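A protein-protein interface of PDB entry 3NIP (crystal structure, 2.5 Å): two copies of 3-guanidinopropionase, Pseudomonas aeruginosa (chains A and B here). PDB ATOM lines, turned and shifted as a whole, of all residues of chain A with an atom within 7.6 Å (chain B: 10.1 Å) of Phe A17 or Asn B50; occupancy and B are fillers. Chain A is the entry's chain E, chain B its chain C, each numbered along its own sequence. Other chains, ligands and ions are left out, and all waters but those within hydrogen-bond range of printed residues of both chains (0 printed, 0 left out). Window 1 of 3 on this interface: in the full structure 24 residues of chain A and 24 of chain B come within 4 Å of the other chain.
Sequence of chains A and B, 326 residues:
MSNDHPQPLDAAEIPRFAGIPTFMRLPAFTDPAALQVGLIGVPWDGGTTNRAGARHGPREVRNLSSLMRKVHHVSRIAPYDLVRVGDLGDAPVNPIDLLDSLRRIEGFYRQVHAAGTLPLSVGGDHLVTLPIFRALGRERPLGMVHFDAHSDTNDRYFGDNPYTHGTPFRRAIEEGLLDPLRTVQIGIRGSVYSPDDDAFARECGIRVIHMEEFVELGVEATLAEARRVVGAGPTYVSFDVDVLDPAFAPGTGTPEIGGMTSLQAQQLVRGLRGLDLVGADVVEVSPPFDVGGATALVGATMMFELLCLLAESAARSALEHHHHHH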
ATOM      1  N   ILE A  14      31.826  13.423  37.293  1.00  0.00           N
ATOM      2  CA  ILE A  14      32.908  13.420  36.306  1.00  0.00           C
ATOM      3  C   ILE A  14      32.332  13.455  34.879  1.00  0.00           C
ATOM      4  O   ILE A  14      31.659  12.518  34.454  1.00  0.00           O
ATOM      5  CB  ILE A  14      33.861  12.193  36.476  1.00  0.00           C
ATOM      6  CG1 ILE A  14      34.183  11.930  37.956  1.00  0.00           C
ATOM      7  CG2 ILE A  14      35.149  12.398  35.684  1.00  0.00           C
ATOM      8  CD1 ILE A  14      34.754  10.522  38.249  1.00  0.00           C
ATOM      9  N   PRO A  15      32.593  14.544  34.135  1.00  0.00           N
ATOM     10  CA  PRO A  15      31.968  14.697  32.819  1.00  0.00           C
ATOM     11  C   PRO A  15      32.475  13.702  31.756  1.00  0.00           C
ATOM     12  O   PRO A  15      33.588  13.176  31.848  1.00  0.00           O
ATOM     13  CB  PRO A  15      32.303  16.140  32.443  1.00  0.00           C
ATOM     14  CG  PRO A  15      33.522  16.463  33.209  1.00  0.00           C
ATOM     15  CD  PRO A  15      33.468  15.682  34.473  1.00  0.00           C
ATOM     16  N   ARG A  16      31.647  13.464  30.748  1.00  0.00           N
ATOM     17  CA  ARG A  16      31.874  12.391  29.792  1.00  0.00           C
ATOM     18  C   ARG A  16      33.141  12.537  28.919  1.00  0.00           C
ATOM     19  O   ARG A  16      33.678  11.543  28.433  1.00  0.00           O
ATOM     20  CB  ARG A  16      30.610  12.176  28.962  1.00  0.00           C
ATOM     21  CG  ARG A  16      29.401  11.868  29.842  1.00  0.00           C
ATOM     22  CD  ARG A  16      28.122  11.531  29.084  1.00  0.00           C
ATOM     23  NE  ARG A  16      27.057  11.151  30.019  1.00  0.00           N
ATOM     24  CZ  ARG A  16      26.918   9.933  30.554  1.00  0.00           C
ATOM     25  NH1 ARG A  16      27.767   8.957  30.249  1.00  0.00           N
ATOM     26  NH2 ARG A  16      25.927   9.681  31.405  1.00  0.00           N
ATOM     27  N   PHE A  17      33.632  13.764  28.755  1.00  0.00           N
ATOM     28  CA  PHE A  17      34.879  13.995  28.027  1.00  0.00           C
ATOM     29  C   PHE A  17      36.129  13.733  28.883  1.00  0.00           C
ATOM     30  O   PHE A  17      37.255  13.819  28.381  1.00  0.00           O
ATOM     31  CB  PHE A  17      34.920  15.420  27.453  1.00  0.00           C
ATOM     32  CG  PHE A  17      34.660  16.496  28.475  1.00  0.00           C
ATOM     33  CD1 PHE A  17      35.644  16.882  29.370  1.00  0.00           C
ATOM     34  CD2 PHE A  17      33.421  17.124  28.541  1.00  0.00           C
ATOM     35  CE1 PHE A  17      35.400  17.865  30.310  1.00  0.00           C
ATOM     36  CE2 PHE A  17      33.178  18.113  29.474  1.00  0.00           C
ATOM     37  CZ  PHE A  17      34.175  18.483  30.356  1.00  0.00           C
ATOM     38  N   ALA A  18      35.924  13.420  30.164  1.00  0.00           N
ATOM     39  CA  ALA A  18      37.022  13.222  31.117  1.00  0.00           C
ATOM     40  C   ALA A  18      37.188  11.769  31.546  1.00  0.00           C
ATOM     41  O   ALA A  18      36.292  10.948  31.373  1.00  0.00           O
ATOM     42  CB  ALA A  18      36.828  14.105  32.343  1.00  0.00           C
ATOM     43  N   GLY A  19      38.348  11.461  32.120  1.00  0.00           N
ATOM     44  CA  GLY A  19      38.656  10.096  32.520  1.00  0.00           C
ATOM     45  C   GLY A  19      39.318   9.315  31.403  1.00  0.00           C
ATOM     46  O   GLY A  19      39.105   9.589  30.212  1.00  0.00           O
ATOM     47  N   ILE A  20      40.143   8.351  31.795  1.00  0.00           N
ATOM     48  CA  ILE A  20      40.795   7.458  30.854  1.00  0.00           C
ATOM     49  C   ILE A  20      39.708   6.638  30.133  1.00  0.00           C
ATOM     50  O   ILE A  20      38.794   6.138  30.779  1.00  0.00           O
ATOM     51  CB  ILE A  20      41.887   6.622  31.573  1.00  0.00           C
ATOM     52  CG1 ILE A  20      43.012   7.564  32.022  1.00  0.00           C
ATOM     53  CG2 ILE A  20      42.427   5.477  30.677  1.00  0.00           C
ATOM     54  CD1 ILE A  20      44.171   6.886  32.702  1.00  0.00           C
ATOM     55  N   PRO A  21      39.763   6.576  28.787  1.00  0.00           N
ATOM     56  CA  PRO A  21      38.657   6.019  27.999  1.00  0.00           C
ATOM     57  C   PRO A  21      38.611   4.501  28.029  1.00  0.00           C
ATOM     58  O   PRO A  21      39.418   3.850  27.363  1.00  0.00           O
ATOM     59  CB  PRO A  21      38.971   6.474  26.572  1.00  0.00           C
ATOM     60  CG  PRO A  21      40.137   7.377  26.673  1.00  0.00           C
ATOM     61  CD  PRO A  21      40.843   7.078  27.922  1.00  0.00           C
ATOM     62  N   ARG A  25      33.209   3.539  30.252  1.00  0.00           N
ATOM     63  CA  ARG A  25      33.873   4.184  31.402  1.00  0.00           C
ATOM     64  C   ARG A  25      33.890   3.295  32.668  1.00  0.00           C
ATOM     65  O   ARG A  25      33.879   3.793  33.799  1.00  0.00           O
ATOM     66  CB  ARG A  25      33.260   5.567  31.719  1.00  0.00           C
ATOM     67  CG  ARG A  25      33.042   6.475  30.497  1.00  0.00           C
ATOM     68  CD  ARG A  25      33.430   7.915  30.796  1.00  0.00           C
ATOM     69  NE  ARG A  25      32.445   8.566  31.651  1.00  0.00           N
ATOM     70  CZ  ARG A  25      32.623   9.732  32.269  1.00  0.00           C
ATOM     71  NH1 ARG A  25      33.757  10.406  32.132  1.00  0.00           N
ATOM     72  NH2 ARG A  25      31.653  10.219  33.037  1.00  0.00           N
ATOM     73  N   ASN A  63      36.378   5.236  23.134  1.00  0.00           N
ATOM     74  CA  ASN A  63      36.214   6.692  23.181  1.00  0.00           C
ATOM     75  C   ASN A  63      34.748   7.117  23.168  1.00  0.00           C
ATOM     76  O   ASN A  63      34.307   7.818  24.079  1.00  0.00           O
ATOM     77  CB  ASN A  63      37.017   7.363  22.046  1.00  0.00           C
ATOM     78  CG  ASN A  63      36.837   8.901  21.984  1.00  0.00           C
ATOM     79  OD1 ASN A  63      36.233   9.547  22.871  1.00  0.00           O
ATOM     80  ND2 ASN A  63      37.382   9.496  20.914  1.00  0.00           N
ATOM     81  N   SER A  66      31.831   6.487  25.974  1.00  0.00           N
ATOM     82  CA  SER A  66      31.657   7.613  26.901  1.00  0.00           C
ATOM     83  C   SER A  66      30.287   8.238  26.907  1.00  0.00           C
ATOM     84  O   SER A  66      29.904   8.843  27.912  1.00  0.00           O
ATOM     85  CB  SER A  66      32.633   8.726  26.553  1.00  0.00           C
ATOM     86  OG  SER A  66      33.811   8.573  27.296  1.00  0.00           O
ATOM     87  N   LEU A  67      29.573   8.147  25.785  1.00  0.00           N
ATOM     88  CA  LEU A  67      28.243   8.739  25.670  1.00  0.00           C
ATOM     89  C   LEU A  67      27.132   7.824  26.160  1.00  0.00           C
ATOM     90  O   LEU A  67      25.976   8.236  26.203  1.00  0.00           O
ATOM     91  CB  LEU A  67      27.937   9.158  24.229  1.00  0.00           C
ATOM     92  CG  LEU A  67      28.797  10.237  23.575  1.00  0.00           C
ATOM     93  CD1 LEU A  67      28.304  10.429  22.167  1.00  0.00           C
ATOM     94  CD2 LEU A  67      28.746  11.567  24.354  1.00  0.00           C
ATOM     95  N   ASP B  45      25.849  28.387  23.967  1.00  0.00           N
ATOM     96  CA  ASP B  45      25.964  26.988  24.385  1.00  0.00           C
ATOM     97  C   ASP B  45      26.602  26.819  25.768  1.00  0.00           C
ATOM     98  O   ASP B  45      27.142  25.760  26.078  1.00  0.00           O
ATOM     99  CB  ASP B  45      26.692  26.156  23.325  1.00  0.00           C
ATOM    100  CG  ASP B  45      28.154  26.570  23.132  1.00  0.00           C
ATOM    101  OD1 ASP B  45      28.723  27.324  23.966  1.00  0.00           O
ATOM    102  OD2 ASP B  45      28.732  26.142  22.107  1.00  0.00           O
ATOM    103  N   GLY B  46      26.522  27.860  26.597  1.00  0.00           N
ATOM    104  CA  GLY B  46      27.008  27.786  27.975  1.00  0.00           C
ATOM    105  C   GLY B  46      26.335  26.697  28.799  1.00  0.00           C
ATOM    106  O   GLY B  46      26.850  26.298  29.847  1.00  0.00           O
ATOM    107  N   GLY B  47      25.184  26.207  28.341  1.00  0.00           N
ATOM    108  CA  GLY B  47      24.480  25.148  29.045  1.00  0.00           C
ATOM    109  C   GLY B  47      24.921  23.742  28.663  1.00  0.00           C
ATOM    110  O   GLY B  47      24.313  22.753  29.106  1.00  0.00           O
ATOM    111  N   THR B  48      25.984  23.636  27.862  1.00  0.00           N
ATOM    112  CA  THR B  48      26.385  22.333  27.321  1.00  0.00           C
ATOM    113  C   THR B  48      27.391  21.639  28.229  1.00  0.00           C
ATOM    114  O   THR B  48      28.407  22.219  28.576  1.00  0.00           O
ATOM    115  CB  THR B  48      26.863  22.426  25.833  1.00  0.00           C
ATOM    116  OG1 THR B  48      25.728  22.685  24.997  1.00  0.00           O
ATOM    117  CG2 THR B  48      27.516  21.114  25.360  1.00  0.00           C
ATOM    118  N   THR B  49      27.101  20.395  28.601  1.00  0.00           N
ATOM    119  CA  THR B  49      27.894  19.688  29.608  1.00  0.00           C
ATOM    120  C   THR B  49      28.977  18.790  29.025  1.00  0.00           C
ATOM    121  O   THR B  49      29.863  18.339  29.743  1.00  0.00           O
ATOM    122  CB  THR B  49      26.998  18.851  30.567  1.00  0.00           C
ATOM    123  OG1 THR B  49      26.161  17.974  29.802  1.00  0.00           O
ATOM    124  CG2 THR B  49      26.117  19.761  31.421  1.00  0.00           C
ATOM    125  N   ASN B  50      28.904  18.516  27.727  1.00  0.00           N
ATOM    126  CA  ASN B  50      29.885  17.659  27.074  1.00  0.00           C
ATOM    127  C   ASN B  50      30.310  18.240  25.722  1.00  0.00           C
ATOM    128  O   ASN B  50      31.137  19.140  25.684  1.00  0.00           O
ATOM    129  CB  ASN B  50      29.341  16.235  26.967  1.00  0.00           C
ATOM    130  CG  ASN B  50      30.391  15.224  26.506  1.00  0.00           C
ATOM    131  OD1 ASN B  50      31.583  15.527  26.406  1.00  0.00           O
ATOM    132  ND2 ASN B  50      29.942  14.013  26.223  1.00  0.00           N
ATOM    133  N   ARG B  51      29.745  17.751  24.622  1.00  0.00           N
ATOM    134  CA  ARG B  51      30.180  18.176  23.284  1.00  0.00           C
ATOM    135  C   ARG B  51      29.509  19.486  22.865  1.00  0.00           C
ATOM    136  O   ARG B  51      28.336  19.504  22.498  1.00  0.00           O
ATOM    137  CB  ARG B  51      29.909  17.062  22.265  1.00  0.00           C
ATOM    138  CG  ARG B  51      31.023  16.029  22.149  1.00  0.00           C
ATOM    139  CD  ARG B  51      30.567  14.692  21.580  1.00  0.00           C
ATOM    140  NE  ARG B  51      29.536  14.841  20.553  1.00  0.00           N
ATOM    141  CZ  ARG B  51      29.562  14.288  19.344  1.00  0.00           C
ATOM    142  NH1 ARG B  51      30.564  13.510  18.976  1.00  0.00           N
ATOM    143  NH2 ARG B  51      28.560  14.514  18.503  1.00  0.00           N
ATOM    144  N   ALA B  52      30.247  20.587  22.962  1.00  0.00           N
ATOM    145  CA  ALA B  52      29.724  21.916  22.634  1.00  0.00           C
ATOM    146  C   ALA B  52      29.990  22.312  21.164  1.00  0.00           C
ATOM    147  O   ALA B  52      30.387  21.474  20.349  1.00  0.00           O
ATOM    148  CB  ALA B  52      30.278  22.945  23.591  1.00  0.00           C
ATOM    149  N   GLY B  53      29.738  23.577  20.838  1.00  0.00           N
ATOM    150  CA  GLY B  53      29.868  24.090  19.473  1.00  0.00           C
ATOM    151  C   GLY B  53      28.619  24.752  18.906  1.00  0.00           C
ATOM    152  O   GLY B  53      28.675  25.437  17.883  1.00  0.00           O
ATOM    153  N   ALA B  54      27.483  24.548  19.562  1.00  0.00           N
ATOM    154  CA  ALA B  54      26.215  25.101  19.092  1.00  0.00           C
ATOM    155  C   ALA B  54      26.188  26.634  19.045  1.00  0.00           C
ATOM    156  O   ALA B  54      25.315  27.217  18.406  1.00  0.00           O
ATOM    157  CB  ALA B  54      25.064  24.565  19.919  1.00  0.00           C
ATOM    158  N   ARG B  55      27.127  27.285  19.718  1.00  0.00           N
ATOM    159  CA  ARG B  55      27.264  28.724  19.613  1.00  0.00           C
ATOM    160  C   ARG B  55      27.489  29.182  18.151  1.00  0.00           C
ATOM    161  O   ARG B  55      27.139  30.322  17.792  1.00  0.00           O
ATOM    162  CB  ARG B  55      28.385  29.237  20.531  1.00  0.00           C
ATOM    163  CG  ARG B  55      29.795  28.794  20.117  1.00  0.00           C
ATOM    164  CD  ARG B  55      30.873  29.335  21.037  1.00  0.00           C
ATOM    165  NE  ARG B  55      30.589  28.981  22.430  1.00  0.00           N
ATOM    166  CZ  ARG B  55      31.414  29.206  23.447  1.00  0.00           C
ATOM    167  NH1 ARG B  55      32.603  29.770  23.226  1.00  0.00           N
ATOM    168  NH2 ARG B  55      31.055  28.853  24.676  1.00  0.00           N
ATOM    169  N   ASP B 125      22.308  25.824  22.133  1.00  0.00           N
ATOM    170  CA  ASP B 125      21.814  24.551  22.644  1.00  0.00           C
ATOM    171  C   ASP B 125      20.412  24.722  23.212  1.00  0.00           C
ATOM    172  O   ASP B 125      19.841  25.806  23.096  1.00  0.00           O
ATOM    173  CB  ASP B 125      22.801  23.885  23.607  1.00  0.00           C
ATOM    174  CG  ASP B 125      23.032  24.664  24.885  1.00  0.00           C
ATOM    175  OD1 ASP B 125      22.132  25.389  25.352  1.00  0.00           O
ATOM    176  OD2 ASP B 125      24.138  24.509  25.453  1.00  0.00           O
ATOM    177  N   TYR B 157      22.683  19.777  37.729  1.00  0.00           N
ATOM    178  CA  TYR B 157      23.923  19.197  37.216  1.00  0.00           C
ATOM    179  C   TYR B 157      25.151  19.593  38.027  1.00  0.00           C
ATOM    180  O   TYR B 157      25.281  20.748  38.469  1.00  0.00           O
ATOM    181  CB  TYR B 157      24.134  19.528  35.733  1.00  0.00           C
ATOM    182  CG  TYR B 157      23.234  18.751  34.793  1.00  0.00           C
ATOM    183  CD1 TYR B 157      23.650  17.542  34.225  1.00  0.00           C
ATOM    184  CD2 TYR B 157      21.960  19.224  34.465  1.00  0.00           C
ATOM    185  CE1 TYR B 157      22.810  16.828  33.347  1.00  0.00           C
ATOM    186  CE2 TYR B 157      21.124  18.521  33.595  1.00  0.00           C
ATOM    187  CZ  TYR B 157      21.547  17.334  33.042  1.00  0.00           C
ATOM    188  OH  TYR B 157      20.697  16.657  32.196  1.00  0.00           O
ATOM    189  N   PHE B 158      26.039  18.613  38.212  1.00  0.00           N
ATOM    190  CA  PHE B 158      27.339  18.786  38.876  1.00  0.00           C
ATOM    191  C   PHE B 158      27.230  19.585  40.173  1.00  0.00           C
ATOM    192  O   PHE B 158      27.943  20.560  40.389  1.00  0.00           O
ATOM    193  CB  PHE B 158      28.373  19.387  37.906  1.00  0.00           C
ATOM    194  CG  PHE B 158      28.530  18.608  36.617  1.00  0.00           C
ATOM    195  CD1 PHE B 158      29.395  17.508  36.552  1.00  0.00           C
ATOM    196  CD2 PHE B 158      27.809  18.976  35.465  1.00  0.00           C
ATOM    197  CE1 PHE B 158      29.539  16.780  35.353  1.00  0.00           C
ATOM    198  CE2 PHE B 158      27.940  18.259  34.264  1.00  0.00           C
ATOM    199  CZ  PHE B 158      28.807  17.163  34.199  1.00  0.00           C
ATOM    200  N   THR B 164      21.082  23.944  32.359  1.00  0.00           N
ATOM    201  CA  THR B 164      21.806  23.284  31.263  1.00  0.00           C
ATOM    202  C   THR B 164      20.859  23.015  30.105  1.00  0.00           C
ATOM    203  O   THR B 164      19.636  23.163  30.224  1.00  0.00           O
ATOM    204  CB  THR B 164      22.441  21.907  31.656  1.00  0.00           C
ATOM    205  OG1 THR B 164      21.426  20.903  31.678  1.00  0.00           O
ATOM    206  CG2 THR B 164      23.156  21.941  32.993  1.00  0.00           C
ATOM    207  N   HIS B 165      21.429  22.579  28.990  1.00  0.00           N
ATOM    208  CA  HIS B 165      20.645  22.185  27.824  1.00  0.00           C
ATOM    209  C   HIS B 165      19.633  21.084  28.167  1.00  0.00           C
ATOM    210  O   HIS B 165      18.652  20.890  27.445  1.00  0.00           O
ATOM    211  CB  HIS B 165      21.566  21.783  26.658  1.00  0.00           C
ATOM    212  CG  HIS B 165      22.293  20.490  26.872  1.00  0.00           C
ATOM    213  ND1 HIS B 165      22.534  19.596  25.851  1.00  0.00           N
ATOM    214  CD2 HIS B 165      22.826  19.938  27.989  1.00  0.00           C
ATOM    215  CE1 HIS B 165      23.180  18.549  26.328  1.00  0.00           C
ATOM    216  NE2 HIS B 165      23.362  18.729  27.626  1.00  0.00           N
ATOM    217  N   GLY B 166      19.868  20.385  29.278  1.00  0.00           N
ATOM    218  CA  GLY B 166      18.955  19.343  29.755  1.00  0.00           C
ATOM    219  C   GLY B 166      17.969  19.715  30.865  1.00  0.00           C
ATOM    220  O   GLY B 166      17.214  18.844  31.338  1.00  0.00           O
ATOM    221  N   THR B 252      25.615  17.606  15.973  1.00  0.00           N
ATOM    222  CA  THR B 252      24.893  17.886  17.199  1.00  0.00           C
ATOM    223  C   THR B 252      25.634  17.295  18.398  1.00  0.00           C
ATOM    224  O   THR B 252      26.317  16.282  18.264  1.00  0.00           O
ATOM    225  CB  THR B 252      23.456  17.365  17.110  1.00  0.00           C
ATOM    226  OG1 THR B 252      22.672  18.033  18.090  1.00  0.00           O
ATOM    227  CG2 THR B 252      23.389  15.850  17.338  1.00  0.00           C
ATOM    228  N   GLY B 253      25.482  17.909  19.566  1.00  0.00           N
ATOM    229  CA  GLY B 253      26.289  17.555  20.724  1.00  0.00           C
ATOM    230  C   GLY B 253      25.969  16.230  21.384  1.00  0.00           C
ATOM    231  O   GLY B 253      26.879  15.502  21.785  1.00  0.00           O
ATOM    232  N   THR B 254      24.684  15.905  21.498  1.00  0.00           N
ATOM    233  CA  THR B 254      24.270  14.693  22.200  1.00  0.00           C
ATOM    234  C   THR B 254      23.427  13.774  21.315  1.00  0.00           C
ATOM    235  O   THR B 254      22.211  13.643  21.517  1.00  0.00           O
ATOM    236  CB  THR B 254      23.510  15.013  23.515  1.00  0.00           C
ATOM    237  OG1 THR B 254      24.145  16.111  24.177  1.00  0.00           O
ATOM    238  CG2 THR B 254      23.511  13.816  24.454  1.00  0.00           C
ATOM    239  N   PRO B 255      24.079  13.090  20.368  1.00  0.00           N
ATOM    240  CA  PRO B 255      23.402  12.194  19.447  1.00  0.00           C
ATOM    241  C   PRO B 255      22.911  10.917  20.129  1.00  0.00           C
ATOM    242  O   PRO B 255      23.522  10.447  21.097  1.00  0.00           O
ATOM    243  CB  PRO B 255      24.492  11.856  18.438  1.00  0.00           C
ATOM    244  CG  PRO B 255      25.770  11.956  19.239  1.00  0.00           C
ATOM    245  CD  PRO B 255      25.537  13.111  20.151  1.00  0.00           C
ATOM    246  N   GLU B 256      21.800  10.382  19.634  1.00  0.00           N
ATOM    247  CA  GLU B 256      21.315   9.085  20.045  1.00  0.00           C
ATOM    248  C   GLU B 256      20.901   8.437  18.750  1.00  0.00           C
ATOM    249  O   GLU B 256      20.062   8.995  18.024  1.00  0.00           O
ATOM    250  CB  GLU B 256      20.095   9.190  20.981  1.00  0.00           C
ATOM    251  CG  GLU B 256      20.247  10.142  22.171  1.00  0.00           C
ATOM    252  CD  GLU B 256      21.208   9.650  23.251  1.00  0.00           C
ATOM    253  OE1 GLU B 256      21.579   8.456  23.269  1.00  0.00           O
ATOM    254  OE2 GLU B 256      21.585  10.472  24.107  1.00  0.00           O
ATOM    255  N   GLU B 284      20.327  23.149  18.631  1.00  0.00           N
ATOM    256  CA  GLU B 284      21.344  22.113  18.825  1.00  0.00           C
ATOM    257  C   GLU B 284      22.149  21.803  17.575  1.00  0.00           C
ATOM    258  O   GLU B 284      22.820  20.775  17.518  1.00  0.00           O
ATOM    259  CB  GLU B 284      20.786  20.832  19.479  1.00  0.00           C
ATOM    260  CG  GLU B 284      20.290  20.999  20.933  1.00  0.00           C
ATOM    261  CD  GLU B 284      21.404  21.100  21.989  1.00  0.00           C
ATOM    262  OE1 GLU B 284      22.599  21.101  21.638  1.00  0.00           O
ATOM    263  OE2 GLU B 284      21.076  21.185  23.193  1.00  0.00           O
ATOM    264  N   SER B 286      25.354  22.078  15.722  1.00  0.00           N
ATOM    265  CA  SER B 286      26.708  22.258  16.237  1.00  0.00           C
ATOM    266  C   SER B 286      27.727  22.074  15.102  1.00  0.00           C
ATOM    267  O   SER B 286      28.121  20.944  14.807  1.00  0.00           O
ATOM    268  CB  SER B 286      26.950  21.240  17.363  1.00  0.00           C
ATOM    269  OG  SER B 286      28.179  21.475  18.036  1.00  0.00           O
ATOM    270  N   PRO B 288      31.004  22.355  14.689  1.00  0.00           N
ATOM    271  CA  PRO B 288      32.270  21.630  14.812  1.00  0.00           C
ATOM    272  C   PRO B 288      32.128  20.120  14.696  1.00  0.00           C
ATOM    273  O   PRO B 288      33.111  19.428  14.430  1.00  0.00           O
ATOM    274  CB  PRO B 288      32.764  22.023  16.203  1.00  0.00           C
ATOM    275  CG  PRO B 288      32.183  23.400  16.402  1.00  0.00           C
ATOM    276  CD  PRO B 288      30.810  23.292  15.817  1.00  0.00           C
ATOM    277  N   PHE B 289      30.913  19.611  14.871  1.00  0.00           N
ATOM    278  CA  PHE B 289      30.670  18.182  14.694  1.00  0.00           C
ATOM    279  C   PHE B 289      29.890  17.901  13.412  1.00  0.00           C
ATOM    280  O   PHE B 289      29.458  16.771  13.173  1.00  0.00           O
ATOM    281  CB  PHE B 289      29.979  17.585  15.936  1.00  0.00           C
ATOM    282  CG  PHE B 289      30.820  17.668  17.173  1.00  0.00           C
ATOM    283  CD1 PHE B 289      31.787  16.690  17.443  1.00  0.00           C
ATOM    284  CD2 PHE B 289      30.687  18.740  18.050  1.00  0.00           C
ATOM    285  CE1 PHE B 289      32.590  16.769  18.572  1.00  0.00           C
ATOM    286  CE2 PHE B 289      31.491  18.827  19.189  1.00  0.00           C
ATOM    287  CZ  PHE B 289      32.441  17.848  19.447  1.00  0.00           C
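O of Ser A66 is in hydrogen-bond range of NH1 of Arg A16 (3.2 Å).
NH1 of Arg A25 lies within hydrogen-bond range of O of Pro A15.
CE1 of Phe B158 touches N of Pro A15, 3.98 Å away.
Arg A16 touches Asn B50 (CB to ND2, 3.4 Å).
Thr B49 touches Phe A17 (O to CE2, 3.3 Å).
Phe A17 touches Asn B50.
CD2 of Leu A67 touches ND2 of Asn B50 (3.3 Å).
Pro A15 touches just one residue of chain B: Phe B158.
Of the printed residues of chain B, Arg A16 touches Asn B50.
Of the printed residues of chain B, Phe A17 touches Thr B49 and Asn B50.
No residue of chain B comes within 4 Å of Ala A18.
Of the printed residues of chain B, Leu A67 touches Asn B50 (3.3 Å).
Printed residues of chain A within 4 Å of Thr B49: Phe A17 (3.3 Å).
Of chain A, only Arg A16, Phe A17 and Leu A67 come within 4 Å of Asn B50.
Of the printed residues of chain A, Phe B158 touches Pro A15.
Thr B254 touches none of the printed residues of chain A.
The nearest residue of chain B that does not touch Phe A17 is Arg B51 (5.4 Å).
Printed residues of chain A that touch a printed residue of chain B: Pro A15, Arg A16, Phe A17 and Leu A67.
Printed residues of chain B that touch a printed residue of chain A: Thr B49, Asn B50 and Phe B158.
Hydrophobic or aromatic side chains of chain B that line the printed part of chain A: Phe B158.
No position is printed for both chains.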
